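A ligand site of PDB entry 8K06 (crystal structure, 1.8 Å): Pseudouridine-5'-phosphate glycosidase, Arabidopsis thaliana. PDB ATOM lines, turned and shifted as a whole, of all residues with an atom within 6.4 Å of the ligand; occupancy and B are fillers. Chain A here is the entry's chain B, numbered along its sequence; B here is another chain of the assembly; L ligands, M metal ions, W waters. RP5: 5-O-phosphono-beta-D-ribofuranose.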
ATOM      1  N   THR A  52      14.867 -16.231 -15.507  1.00  0.00           N
ATOM      2  CA  THR A  52      16.225 -16.544 -15.994  1.00  0.00           C
ATOM      3  C   THR A  52      16.296 -16.641 -17.513  1.00  0.00           C
ATOM      4  O   THR A  52      17.373 -16.489 -18.090  1.00  0.00           O
ATOM      5  CB  THR A  52      16.834 -17.844 -15.405  1.00  0.00           C
ATOM      6  OG1 THR A  52      15.941 -18.935 -15.606  1.00  0.00           O
ATOM      7  CG2 THR A  52      17.114 -17.672 -13.925  1.00  0.00           C
ATOM      8  N   LYS A 112      21.697 -15.690 -11.106  1.00  0.00           N
ATOM      9  CA  LYS A 112      20.831 -16.770 -11.502  1.00  0.00           C
ATOM     10  C   LYS A 112      20.390 -17.449 -10.219  1.00  0.00           C
ATOM     11  O   LYS A 112      21.191 -18.055  -9.505  1.00  0.00           O
ATOM     12  CB  LYS A 112      21.540 -17.729 -12.482  1.00  0.00           C
ATOM     13  CG  LYS A 112      20.759 -18.969 -12.855  1.00  0.00           C
ATOM     14  CD  LYS A 112      21.541 -19.690 -13.936  1.00  0.00           C
ATOM     15  CE  LYS A 112      20.989 -21.040 -14.253  1.00  0.00           C
ATOM     16  NZ  LYS A 112      21.755 -21.675 -15.392  1.00  0.00           N
ATOM     17  N   THR A 113      19.098 -17.372  -9.929  1.00  0.00           N
ATOM     18  CA  THR A 113      18.626 -17.688  -8.589  1.00  0.00           C
ATOM     19  C   THR A 113      17.783 -18.943  -8.561  1.00  0.00           C
ATOM     20  O   THR A 113      16.630 -18.925  -8.993  1.00  0.00           O
ATOM     21  CB  THR A 113      17.790 -16.493  -7.997  1.00  0.00           C
ATOM     22  OG1 THR A 113      18.564 -15.304  -8.039  1.00  0.00           O
ATOM     23  CG2 THR A 113      17.407 -16.769  -6.541  1.00  0.00           C
ATOM     24  N   ALA A 114      18.362 -20.053  -8.073  1.00  0.00           N
ATOM     25  CA  ALA A 114      17.598 -21.270  -7.795  1.00  0.00           C
ATOM     26  C   ALA A 114      16.864 -21.096  -6.472  1.00  0.00           C
ATOM     27  O   ALA A 114      17.131 -20.129  -5.743  1.00  0.00           O
ATOM     28  CB  ALA A 114      18.526 -22.509  -7.743  1.00  0.00           C
ATOM     29  N   GLY A 115      15.970 -22.024  -6.152  1.00  0.00           N
ATOM     30  CA  GLY A 115      15.203 -21.951  -4.916  1.00  0.00           C
ATOM     31  C   GLY A 115      16.138 -21.780  -3.711  1.00  0.00           C
ATOM     32  O   GLY A 115      15.883 -20.967  -2.839  1.00  0.00           O
ATOM     33  N   ARG A 116      17.252 -22.507  -3.720  1.00  0.00           N
ATOM     34  CA  ARG A 116      18.199 -22.478  -2.599  1.00  0.00           C
ATOM     35  C   ARG A 116      18.987 -21.165  -2.482  1.00  0.00           C
ATOM     36  O   ARG A 116      19.636 -20.912  -1.461  1.00  0.00           O
ATOM     37  CB  ARG A 116      19.167 -23.669  -2.759  1.00  0.00           C
ATOM     38  CG  ARG A 116      20.045 -23.542  -3.995  1.00  0.00           C
ATOM     39  CD  ARG A 116      21.153 -24.615  -4.100  1.00  0.00           C
ATOM     40  NE  ARG A 116      21.821 -24.370  -5.378  1.00  0.00           N
ATOM     41  CZ  ARG A 116      21.398 -24.872  -6.544  1.00  0.00           C
ATOM     42  NH1 ARG A 116      20.370 -25.720  -6.598  1.00  0.00           N
ATOM     43  NH2 ARG A 116      22.034 -24.536  -7.660  1.00  0.00           N
ATOM     44  N   ASP A 117      18.903 -20.324  -3.491  1.00  0.00           N
ATOM     45  CA  ASP A 117      19.583 -19.043  -3.499  1.00  0.00           C
ATOM     46  C   ASP A 117      18.675 -17.879  -3.062  1.00  0.00           C
ATOM     47  O   ASP A 117      19.156 -16.756  -2.898  1.00  0.00           O
ATOM     48  CB  ASP A 117      20.120 -18.738  -4.905  1.00  0.00           C
ATOM     49  CG  ASP A 117      21.112 -19.793  -5.379  1.00  0.00           C
ATOM     50  OD1 ASP A 117      22.083 -20.110  -4.645  1.00  0.00           O
ATOM     51  OD2 ASP A 117      20.918 -20.297  -6.505  1.00  0.00           O
ATOM     52  N   THR A 131      15.036 -19.197 -11.367  1.00  0.00           N
ATOM     53  CA  THR A 131      14.982 -20.398 -12.200  1.00  0.00           C
ATOM     54  C   THR A 131      13.644 -21.087 -12.013  1.00  0.00           C
ATOM     55  O   THR A 131      12.786 -20.575 -11.309  1.00  0.00           O
ATOM     56  CB  THR A 131      16.092 -21.395 -11.799  1.00  0.00           C
ATOM     57  OG1 THR A 131      15.838 -21.815 -10.457  1.00  0.00           O
ATOM     58  CG2 THR A 131      17.459 -20.739 -11.862  1.00  0.00           C
ATOM     59  N   VAL A 132      13.445 -22.243 -12.640  1.00  0.00           N
ATOM     60  CA  VAL A 132      12.213 -23.007 -12.411  1.00  0.00           C
ATOM     61  C   VAL A 132      11.982 -23.344 -10.929  1.00  0.00           C
ATOM     62  O   VAL A 132      10.863 -23.162 -10.415  1.00  0.00           O
ATOM     63  CB  VAL A 132      12.202 -24.288 -13.270  1.00  0.00           C
ATOM     64  CG1 VAL A 132      11.147 -25.283 -12.756  1.00  0.00           C
ATOM     65  CG2 VAL A 132      11.954 -23.911 -14.731  1.00  0.00           C
ATOM     66  N   SER A 133      13.015 -23.820 -10.222  1.00  0.00           N
ATOM     67  CA  SER A 133      12.833 -24.190  -8.817  1.00  0.00           C
ATOM     68  C   SER A 133      12.465 -22.989  -7.943  1.00  0.00           C
ATOM     69  O   SER A 133      11.687 -23.137  -6.998  1.00  0.00           O
ATOM     70  CB  SER A 133      14.083 -24.893  -8.249  1.00  0.00           C
ATOM     71  OG  SER A 133      15.221 -24.024  -8.241  1.00  0.00           O
ATOM     72  N   ILE A 152      12.652 -27.518 -18.720  1.00  0.00           N
ATOM     73  CA  ILE A 152      12.958 -27.699 -17.309  1.00  0.00           C
ATOM     74  C   ILE A 152      14.403 -28.242 -17.194  1.00  0.00           C
ATOM     75  O   ILE A 152      14.877 -28.923 -18.112  1.00  0.00           O
ATOM     76  CB  ILE A 152      11.896 -28.619 -16.633  1.00  0.00           C
ATOM     77  CG1 ILE A 152      12.071 -28.622 -15.121  1.00  0.00           C
ATOM     78  CG2 ILE A 152      11.946 -30.070 -17.210  1.00  0.00           C
ATOM     79  CD1 ILE A 152      10.893 -29.324 -14.372  1.00  0.00           C
ATOM     80  N   GLY A 153      15.097 -27.906 -16.104  1.00  0.00           N
ATOM     81  CA  GLY A 153      16.412 -28.487 -15.823  1.00  0.00           C
ATOM     82  C   GLY A 153      16.239 -29.990 -15.596  1.00  0.00           C
ATOM     83  O   GLY A 153      15.117 -30.465 -15.375  1.00  0.00           O
ATOM     84  N   GLY A 154      17.323 -30.761 -15.626  1.00  0.00           N
ATOM     85  CA  GLY A 154      17.137 -32.189 -15.498  1.00  0.00           C
ATOM     86  C   GLY A 154      18.386 -32.892 -15.006  1.00  0.00           C
ATOM     87  O   GLY A 154      19.207 -32.284 -14.315  1.00  0.00           O
ATOM     88  N   HIS A 156      21.883 -34.194 -15.682  1.00  0.00           N
ATOM     89  CA  HIS A 156      22.898 -33.835 -16.673  1.00  0.00           C
ATOM     90  C   HIS A 156      23.550 -35.072 -17.227  1.00  0.00           C
ATOM     91  O   HIS A 156      23.492 -36.145 -16.623  1.00  0.00           O
ATOM     92  CB  HIS A 156      23.949 -32.918 -16.050  1.00  0.00           C
ATOM     93  CG  HIS A 156      23.441 -31.548 -15.764  1.00  0.00           C
ATOM     94  ND1 HIS A 156      23.823 -30.437 -16.485  1.00  0.00           N
ATOM     95  CD2 HIS A 156      22.529 -31.106 -14.858  1.00  0.00           C
ATOM     96  CE1 HIS A 156      23.184 -29.375 -16.027  1.00  0.00           C
ATOM     97  NE2 HIS A 156      22.395 -29.756 -15.042  1.00  0.00           N
ATOM     98  N   ASP A 164      25.274 -34.443 -10.972  1.00  0.00           N
ATOM     99  CA  ASP A 164      24.757 -33.120 -11.320  1.00  0.00           C
ATOM    100  C   ASP A 164      23.312 -33.230 -11.819  1.00  0.00           C
ATOM    101  O   ASP A 164      23.055 -33.630 -12.953  1.00  0.00           O
ATOM    102  CB  ASP A 164      25.655 -32.468 -12.373  1.00  0.00           C
ATOM    103  CG  ASP A 164      25.291 -31.010 -12.644  1.00  0.00           C
ATOM    104  OD1 ASP A 164      24.377 -30.491 -11.971  1.00  0.00           O
ATOM    105  OD2 ASP A 164      25.953 -30.374 -13.500  1.00  0.00           O
ATOM    106  N   ILE A 165      22.377 -32.874 -10.932  1.00  0.00           N
ATOM    107  CA  ILE A 165      20.949 -33.001 -11.189  1.00  0.00           C
ATOM    108  C   ILE A 165      20.217 -31.736 -10.734  1.00  0.00           C
ATOM    109  O   ILE A 165      20.373 -31.290  -9.590  1.00  0.00           O
ATOM    110  CB  ILE A 165      20.365 -34.216 -10.446  1.00  0.00           C
ATOM    111  CG1 ILE A 165      21.053 -35.510 -10.912  1.00  0.00           C
ATOM    112  CG2 ILE A 165      18.835 -34.300 -10.649  1.00  0.00           C
ATOM    113  CD1 ILE A 165      20.557 -36.773 -10.175  1.00  0.00           C
ATOM    114  N   SER A 166      19.402 -31.164 -11.607  1.00  0.00           N
ATOM    115  CA  SER A 166      18.750 -29.902 -11.334  1.00  0.00           C
ATOM    116  C   SER A 166      17.784 -29.977 -10.160  1.00  0.00           C
ATOM    117  O   SER A 166      16.995 -30.923 -10.045  1.00  0.00           O
ATOM    118  CB  SER A 166      17.985 -29.423 -12.579  1.00  0.00           C
ATOM    119  OG  SER A 166      17.303 -28.241 -12.271  1.00  0.00           O
ATOM    120  N   SER A 167      17.844 -28.966  -9.284  1.00  0.00           N
ATOM    121  CA  SER A 167      16.872 -28.886  -8.195  1.00  0.00           C
ATOM    122  C   SER A 167      15.464 -28.635  -8.730  1.00  0.00           C
ATOM    123  O   SER A 167      14.509 -28.699  -7.975  1.00  0.00           O
ATOM    124  CB  SER A 167      17.248 -27.803  -7.152  1.00  0.00           C
ATOM    125  OG  SER A 167      17.213 -26.492  -7.717  1.00  0.00           O
ATOM    126  N   ASP A 168      15.326 -28.332 -10.018  1.00  0.00           N
ATOM    127  CA  ASP A 168      13.981 -28.218 -10.587  1.00  0.00           C
ATOM    128  C   ASP A 168      13.159 -29.487 -10.331  1.00  0.00           C
ATOM    129  O   ASP A 168      11.951 -29.408 -10.106  1.00  0.00           O
ATOM    130  CB  ASP A 168      14.006 -27.972 -12.104  1.00  0.00           C
ATOM    131  CG  ASP A 168      14.593 -26.619 -12.472  1.00  0.00           C
ATOM    132  OD1 ASP A 168      14.826 -25.781 -11.558  1.00  0.00           O
ATOM    133  OD2 ASP A 168      14.820 -26.404 -13.692  1.00  0.00           O
ATOM    134  N   LEU A 188      20.696 -32.251 -21.800  1.00  0.00           N
ATOM    135  CA  LEU A 188      20.513 -33.081 -20.606  1.00  0.00           C
ATOM    136  C   LEU A 188      20.279 -34.548 -20.996  1.00  0.00           C
ATOM    137  O   LEU A 188      20.120 -34.855 -22.177  1.00  0.00           O
ATOM    138  CB  LEU A 188      19.347 -32.548 -19.798  1.00  0.00           C
ATOM    139  CG  LEU A 188      19.544 -31.123 -19.286  1.00  0.00           C
ATOM    140  CD1 LEU A 188      18.213 -30.478 -18.954  1.00  0.00           C
ATOM    141  CD2 LEU A 188      20.464 -31.155 -18.039  1.00  0.00           C
ATOM    142  N   GLY A 285      29.652 -24.824 -14.261  1.00  0.00           N
ATOM    143  CA  GLY A 285      28.733 -24.121 -13.389  1.00  0.00           C
ATOM    144  C   GLY A 285      27.737 -23.283 -14.156  1.00  0.00           C
ATOM    145  O   GLY A 285      27.235 -23.692 -15.215  1.00  0.00           O
ATOM    146  N   ASN A 286      27.450 -22.095 -13.635  1.00  0.00           N
ATOM    147  CA  ASN A 286      26.422 -21.241 -14.181  1.00  0.00           C
ATOM    148  C   ASN A 286      26.789 -20.651 -15.556  1.00  0.00           C
ATOM    149  O   ASN A 286      25.945 -20.056 -16.244  1.00  0.00           O
ATOM    150  CB  ASN A 286      26.122 -20.122 -13.176  1.00  0.00           C
ATOM    151  CG  ASN A 286      27.326 -19.179 -12.992  1.00  0.00           C
ATOM    152  OD1 ASN A 286      28.452 -19.518 -13.345  1.00  0.00           O
ATOM    153  ND2 ASN A 286      27.073 -17.995 -12.434  1.00  0.00           N
ATOM    154  N   GLU A 288      27.896 -22.585 -17.997  1.00  0.00           N
ATOM    155  CA  GLU A 288      27.802 -23.663 -18.971  1.00  0.00           C
ATOM    156  C   GLU A 288      26.591 -23.571 -19.892  1.00  0.00           C
ATOM    157  O   GLU A 288      26.727 -23.598 -21.115  1.00  0.00           O
ATOM    158  CB  GLU A 288      27.751 -25.017 -18.271  1.00  0.00           C
ATOM    159  CG  GLU A 288      27.792 -26.179 -19.261  1.00  0.00           C
ATOM    160  CD  GLU A 288      27.834 -27.520 -18.568  1.00  0.00           C
ATOM    161  OE1 GLU A 288      26.747 -28.003 -18.190  1.00  0.00           O
ATOM    162  OE2 GLU A 288      28.937 -28.089 -18.412  1.00  0.00           O
ATOM    163  N   THR A 289      25.402 -23.476 -19.308  1.00  0.00           N
ATOM    164  CA  THR A 289      24.185 -23.433 -20.102  1.00  0.00           C
ATOM    165  C   THR A 289      24.182 -22.240 -21.059  1.00  0.00           C
ATOM    166  O   THR A 289      23.834 -22.399 -22.221  1.00  0.00           O
ATOM    167  CB  THR A 289      22.948 -23.402 -19.222  1.00  0.00           C
ATOM    168  OG1 THR A 289      22.841 -24.658 -18.531  1.00  0.00           O
ATOM    169  CG2 THR A 289      21.695 -23.213 -20.058  1.00  0.00           C
ATOM    170  N   PRO A 290      24.570 -21.050 -20.579  1.00  0.00           N
ATOM    171  CA  PRO A 290      24.647 -19.903 -21.496  1.00  0.00           C
ATOM    172  C   PRO A 290      25.671 -20.118 -22.629  1.00  0.00           C
ATOM    173  O   PRO A 290      25.426 -19.711 -23.774  1.00  0.00           O
ATOM    174  CB  PRO A 290      25.086 -18.757 -20.579  1.00  0.00           C
ATOM    175  CG  PRO A 290      24.561 -19.152 -19.232  1.00  0.00           C
ATOM    176  CD  PRO A 290      24.739 -20.647 -19.172  1.00  0.00           C
ATOM    177  N   GLU B 198      22.914 -29.272  -3.642  1.00  0.00           N
ATOM    178  CA  GLU B 198      22.253 -28.361  -4.595  1.00  0.00           C
ATOM    179  C   GLU B 198      20.928 -28.939  -5.038  1.00  0.00           C
ATOM    180  O   GLU B 198      19.914 -28.241  -5.087  1.00  0.00           O
ATOM    181  CB  GLU B 198      23.108 -28.124  -5.852  1.00  0.00           C
ATOM    182  CG  GLU B 198      24.312 -27.253  -5.654  1.00  0.00           C
ATOM    183  CD  GLU B 198      24.972 -26.822  -6.961  1.00  0.00           C
ATOM    184  OE1 GLU B 198      26.045 -26.177  -6.891  1.00  0.00           O
ATOM    185  OE2 GLU B 198      24.412 -27.120  -8.032  1.00  0.00           O
ATOM    186  N   THR B 199      20.943 -30.216  -5.372  1.00  0.00           N
ATOM    187  CA  THR B 199      19.722 -30.907  -5.824  1.00  0.00           C
ATOM    188  C   THR B 199      18.639 -30.903  -4.723  1.00  0.00           C
ATOM    189  O   THR B 199      17.437 -30.747  -5.027  1.00  0.00           O
ATOM    190  CB  THR B 199      20.033 -32.351  -6.230  1.00  0.00           C
ATOM    191  OG1 THR B 199      21.093 -32.337  -7.200  1.00  0.00           O
ATOM    192  CG2 THR B 199      18.805 -33.048  -6.830  1.00  0.00           C
HETATM  193  C1  RP5 L   1      18.895 -24.598 -14.503  1.00  0.00           C
HETATM  194  O4  RP5 L   1      18.942 -25.844 -13.746  1.00  0.00           O
HETATM  195  C2  RP5 L   1      20.308 -24.174 -14.704  1.00  0.00           C
HETATM  196  O2  RP5 L   1      20.597 -24.004 -16.109  1.00  0.00           O
HETATM  197  C3  RP5 L   1      21.193 -25.190 -14.098  1.00  0.00           C
HETATM  198  O3  RP5 L   1      22.300 -25.505 -14.988  1.00  0.00           O
HETATM  199  C4  RP5 L   1      20.301 -26.364 -13.900  1.00  0.00           C
HETATM  200  C5  RP5 L   1      20.684 -27.123 -12.679  1.00  0.00           C
HETATM  201  O5  RP5 L   1      19.674 -26.845 -11.735  1.00  0.00           O
HETATM  202  P'  RP5 L   1      19.973 -26.066 -10.394  1.00  0.00           P
HETATM  203  O1X RP5 L   1      19.195 -24.806 -10.263  1.00  0.00           O
HETATM  204  O2X RP5 L   1      21.355 -25.556 -10.214  1.00  0.00           O
HETATM  205  O3X RP5 L   1      19.701 -26.884  -9.214  1.00  0.00           O
HETATM  206  O1  RP5 L   1      18.195 -23.617 -13.827  1.00  0.00           O
HETATM  207 MN    MN M   1      23.595 -28.455 -11.629  1.00  0.00          MN
HETATM  208  O   HOH W   1      22.233 -28.825  -9.609  1.00  0.00           O
HETATM  209  O   HOH W   2      21.058 -22.769 -11.365  1.00  0.00           O
HETATM  210  O   HOH W   3      16.759 -24.318 -10.488  1.00  0.00           O
HETATM  211  O   HOH W   4      24.682 -23.855 -16.251  1.00  0.00           O
HETATM  212  O   HOH W   5      19.515 -28.823 -15.635  1.00  0.00           O
HETATM  213  O   HOH W   6      23.461 -26.281 -11.226  1.00  0.00           O
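OG of Ser 167 sits at hydrogen-bond distance from OG of Ser 133 (3.2 Å). The side-chain hydroxyl of Ser 166 lies close to the backbone NH of Asp 168 (3.0 Å). The backbone NH (N) of Ser 166 sits at hydrogen-bond distance from the backbone carbonyl oxygen (O) of Gly 154. NH2 of Arg 116 is in salt-bridge range of OE2 of Glu 198 of chain B (3.5 Å). OD2 of Asp 117 lies within hydrogen-bond range of N of Ala 114. OG1 of Thr 131 is in hydrogen-bond range of OG of Ser 133, at 3.2 Å. The backbone NH of Thr 131 is in hydrogen-bond range of the backbone carbonyl oxygen of Thr 113. N of His 156 lies within hydrogen-bond range of O of Asp 164 (3.0 Å).
Water W6 lies within hydrogen-bond range of an oxygen (O2X) of the ligand (2.4 Å) and the side-chain carboxylate (OE2) of Glu 198 of chain B (3.4 Å). Water W3 lies within hydrogen-bond range of O1X of the ligand (2.5 Å), OD1 of Asp 168 (2.6 Å), OG1 of Thr 131 (2.7 Å) and OG of Ser 133 (2.7 Å). Water W5 lies within hydrogen-bond range of N of Gly 154 (2.9 Å) and NE2 of His 156 (3.1 Å). Water W4 lies within hydrogen-bond range of the backbone carbonyl oxygen (O) of Gly 285 (2.8 Å), the side-chain hydroxyl (OG1) of Thr 289 (3.0 Å) and an oxygen (O3) of the ligand (3.2 Å). Water W1 lies within hydrogen-bond range of O of Ile 165 (3.1 Å), OE2 of Glu 198 of chain B (3.2 Å) and O3X of the ligand (3.2 Å).
Residues that only touch the ligand: Ala 114 (3.5 Å), Thr 131 (3.6 Å) and His 156 (3.9 Å). Within 4 Å of the ligand: Lys 112, Ala 114, Arg 116, Thr 131, His 156, Ser 166, Ser 167 and Thr 289. The nearest printed residue that does not touch the ligand is Glu 198 of chain B (4.1 Å).
O2 of the ligand is in hydrogen-bond range of NZ of Lys 112 (2.7 Å). An oxygen (O3X) of the ligand lies within hydrogen-bond range of the backbone NH (N) of Ser 167 (2.8 Å). An oxygen (O3X) of the ligand is in hydrogen-bond range of the side-chain hydroxyl (OG) of Ser 167, 2.9 Å away. O5 of the ligand sits at hydrogen-bond distance from OG of Ser 166, 2.8 Å away. An oxygen (O2X) of the ligand lies within salt-bridge range of the guanidinium group of Arg 116, at 2.8 Å. The side-chain hydroxyl of Thr 289 sits at hydrogen-bond distance from an oxygen (O2) of the ligand, at 3.4 Å.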
